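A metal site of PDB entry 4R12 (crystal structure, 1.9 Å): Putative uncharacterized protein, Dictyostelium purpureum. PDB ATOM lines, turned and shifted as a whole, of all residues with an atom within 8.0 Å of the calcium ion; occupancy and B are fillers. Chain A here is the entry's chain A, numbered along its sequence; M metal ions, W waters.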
ATOM      1  N   TYR A 510     -20.520  30.834   0.018  1.00  0.00           N
ATOM      2  CA  TYR A 510     -20.455  29.751  -0.964  1.00  0.00           C
ATOM      3  C   TYR A 510     -18.999  29.313  -1.160  1.00  0.00           C
ATOM      4  O   TYR A 510     -18.681  28.121  -1.119  1.00  0.00           O
ATOM      5  CB  TYR A 510     -21.077  30.191  -2.290  1.00  0.00           C
ATOM      6  CG  TYR A 510     -21.277  29.086  -3.312  1.00  0.00           C
ATOM      7  CD1 TYR A 510     -20.197  28.616  -4.077  1.00  0.00           C
ATOM      8  CD2 TYR A 510     -22.528  28.514  -3.520  1.00  0.00           C
ATOM      9  CE1 TYR A 510     -20.376  27.603  -5.009  1.00  0.00           C
ATOM     10  CE2 TYR A 510     -22.718  27.495  -4.447  1.00  0.00           C
ATOM     11  CZ  TYR A 510     -21.639  27.043  -5.190  1.00  0.00           C
ATOM     12  OH  TYR A 510     -21.811  26.037  -6.119  1.00  0.00           O
ATOM     13  N   SER A 524     -19.684  32.403 -16.803  1.00  0.00           N
ATOM     14  CA  SER A 524     -20.894  32.732 -16.063  1.00  0.00           C
ATOM     15  C   SER A 524     -21.379  31.493 -15.330  1.00  0.00           C
ATOM     16  O   SER A 524     -20.995  30.379 -15.676  1.00  0.00           O
ATOM     17  CB  SER A 524     -21.989  33.256 -16.986  1.00  0.00           C
ATOM     18  OG  SER A 524     -22.637  32.175 -17.628  1.00  0.00           O
ATOM     19  N   ASP A 525     -22.226  31.679 -14.318  1.00  0.00           N
ATOM     20  CA  ASP A 525     -22.713  30.563 -13.528  1.00  0.00           C
ATOM     21  C   ASP A 525     -23.440  29.521 -14.383  1.00  0.00           C
ATOM     22  O   ASP A 525     -23.372  28.336 -14.090  1.00  0.00           O
ATOM     23  CB  ASP A 525     -23.651  31.050 -12.413  1.00  0.00           C
ATOM     24  CG  ASP A 525     -22.952  31.936 -11.408  1.00  0.00           C
ATOM     25  OD1 ASP A 525     -21.711  31.828 -11.247  1.00  0.00           O
ATOM     26  OD2 ASP A 525     -23.642  32.750 -10.756  1.00  0.00           O
ATOM     27  N   ASN A 526     -24.105  29.956 -15.454  1.00  0.00           N
ATOM     28  CA  ASN A 526     -24.839  29.021 -16.304  1.00  0.00           C
ATOM     29  C   ASN A 526     -23.916  28.070 -17.077  1.00  0.00           C
ATOM     30  O   ASN A 526     -24.375  27.061 -17.629  1.00  0.00           O
ATOM     31  CB  ASN A 526     -25.750  29.774 -17.288  1.00  0.00           C
ATOM     32  CG  ASN A 526     -26.816  30.599 -16.588  1.00  0.00           C
ATOM     33  OD1 ASN A 526     -27.169  30.347 -15.427  1.00  0.00           O
ATOM     34  ND2 ASN A 526     -27.345  31.597 -17.291  1.00  0.00           N
ATOM     35  N   ASP A 527     -22.625  28.375 -17.126  1.00  0.00           N
ATOM     36  CA  ASP A 527     -21.647  27.471 -17.729  1.00  0.00           C
ATOM     37  C   ASP A 527     -21.336  26.280 -16.821  1.00  0.00           C
ATOM     38  O   ASP A 527     -20.745  25.288 -17.270  1.00  0.00           O
ATOM     39  CB  ASP A 527     -20.318  28.197 -18.022  1.00  0.00           C
ATOM     40  CG  ASP A 527     -20.435  29.227 -19.114  1.00  0.00           C
ATOM     41  OD1 ASP A 527     -21.409  29.201 -19.896  1.00  0.00           O
ATOM     42  OD2 ASP A 527     -19.513  30.071 -19.210  1.00  0.00           O
ATOM     43  N   CYS A 528     -21.718  26.400 -15.559  1.00  0.00           N
ATOM     44  CA  CYS A 528     -21.324  25.427 -14.535  1.00  0.00           C
ATOM     45  C   CYS A 528     -22.502  24.541 -14.084  1.00  0.00           C
ATOM     46  O   CYS A 528     -23.425  25.016 -13.429  1.00  0.00           O
ATOM     47  CB  CYS A 528     -20.735  26.152 -13.312  1.00  0.00           C
ATOM     48  SG  CYS A 528     -19.147  27.018 -13.686  1.00  0.00           S
ATOM     49  N   PRO A 529     -22.440  23.241 -14.413  1.00  0.00           N
ATOM     50  CA  PRO A 529     -23.497  22.323 -13.981  1.00  0.00           C
ATOM     51  C   PRO A 529     -23.531  22.178 -12.466  1.00  0.00           C
ATOM     52  O   PRO A 529     -22.505  21.801 -11.887  1.00  0.00           O
ATOM     53  CB  PRO A 529     -23.097  20.998 -14.646  1.00  0.00           C
ATOM     54  CG  PRO A 529     -22.133  21.367 -15.728  1.00  0.00           C
ATOM     55  CD  PRO A 529     -21.405  22.561 -15.193  1.00  0.00           C
ATOM     56  N   SER A 530     -24.666  22.497 -11.843  1.00  0.00           N
ATOM     57  CA  SER A 530     -24.838  22.362 -10.393  1.00  0.00           C
ATOM     58  C   SER A 530     -23.697  23.033  -9.606  1.00  0.00           C
ATOM     59  O   SER A 530     -23.239  22.524  -8.589  1.00  0.00           O
ATOM     60  CB  SER A 530     -24.931  20.889 -10.000  1.00  0.00           C
ATOM     61  OG  SER A 530     -25.788  20.178 -10.885  1.00  0.00           O
ATOM     62  N   SER A 531     -23.254  24.170 -10.106  1.00  0.00           N
ATOM     63  CA  SER A 531     -22.158  24.877  -9.458  1.00  0.00           C
ATOM     64  C   SER A 531     -22.151  26.329  -9.935  1.00  0.00           C
ATOM     65  O   SER A 531     -22.968  26.719 -10.773  1.00  0.00           O
ATOM     66  CB  SER A 531     -20.826  24.183  -9.733  1.00  0.00           C
ATOM     67  OG  SER A 531     -20.690  23.788 -11.097  1.00  0.00           O
ATOM     68  N   LEU A 532     -21.252  27.128  -9.380  1.00  0.00           N
ATOM     69  CA  LEU A 532     -21.171  28.536  -9.722  1.00  0.00           C
ATOM     70  C   LEU A 532     -19.801  28.839 -10.311  1.00  0.00           C
ATOM     71  O   LEU A 532     -18.837  28.137 -10.044  1.00  0.00           O
ATOM     72  CB  LEU A 532     -21.421  29.424  -8.499  1.00  0.00           C
ATOM     73  CG  LEU A 532     -22.788  29.306  -7.822  1.00  0.00           C
ATOM     74  CD1 LEU A 532     -22.883  30.296  -6.650  1.00  0.00           C
ATOM     75  CD2 LEU A 532     -23.925  29.489  -8.827  1.00  0.00           C
ATOM     76  N   CYS A 533     -19.735  29.884 -11.123  1.00  0.00           N
ATOM     77  CA  CYS A 533     -18.469  30.261 -11.736  1.00  0.00           C
ATOM     78  C   CYS A 533     -17.713  31.326 -10.926  1.00  0.00           C
ATOM     79  O   CYS A 533     -18.252  32.402 -10.626  1.00  0.00           O
ATOM     80  CB  CYS A 533     -18.705  30.754 -13.162  1.00  0.00           C
ATOM     81  SG  CYS A 533     -17.154  31.105 -14.012  1.00  0.00           S
ATOM     82  N   CYS A 538     -15.384  26.268 -11.943  1.00  0.00           N
ATOM     83  CA  CYS A 538     -16.706  25.824 -11.485  1.00  0.00           C
ATOM     84  C   CYS A 538     -16.563  25.332 -10.052  1.00  0.00           C
ATOM     85  O   CYS A 538     -15.822  24.377  -9.787  1.00  0.00           O
ATOM     86  CB  CYS A 538     -17.293  24.739 -12.394  1.00  0.00           C
ATOM     87  SG  CYS A 538     -17.876  25.415 -13.962  1.00  0.00           S
ATOM     88  N   VAL A 539     -17.241  26.001  -9.123  1.00  0.00           N
ATOM     89  CA  VAL A 539     -17.054  25.743  -7.703  1.00  0.00           C
ATOM     90  C   VAL A 539     -18.323  25.123  -7.132  1.00  0.00           C
ATOM     91  O   VAL A 539     -19.440  25.591  -7.379  1.00  0.00           O
ATOM     92  CB  VAL A 539     -16.704  27.028  -6.922  1.00  0.00           C
ATOM     93  CG1 VAL A 539     -16.495  26.743  -5.445  1.00  0.00           C
ATOM     94  CG2 VAL A 539     -15.459  27.683  -7.540  1.00  0.00           C
HETATM   95 CA    CA M   1     -24.605  26.893 -12.665  1.00  0.00          CA
HETATM   96  O   HOH W   1     -26.043  28.621 -12.066  1.00  0.00           O
HETATM   97  O   HOH W   2     -26.000  25.975 -14.560  1.00  0.00           O
HETATM   98  O   HOH W   3     -26.006  25.744 -10.942  1.00  0.00           O
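OG of Ser 531 is in hydrogen-bond range of O of Pro 529, at 2.8 Å.
SG of Cys 538 is disulfide-bonded to SG of Cys 528 (2.1 Å).
The side-chain carboxylate (OD1) of Asp 525 is in hydrogen-bond range of the backbone NH (N) of Cys 533, 2.8 Å away.
Of the 13 residues printed, 3 come within 4 Å of the calcium ion.
Water W1 is bound to the calcium ion.
The backbone carbonyl oxygen (O) of Cys 528 is bound to the calcium ion, 2.3 Å away.
The calcium ion is bound by the backbone carbonyl oxygen (O) of Asp 525 (2.4 Å).
Water W3 binds the calcium ion.
O of Ser 531 is bound to the calcium ion.
The calcium ion is bound by water W2 (2.5 Å).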
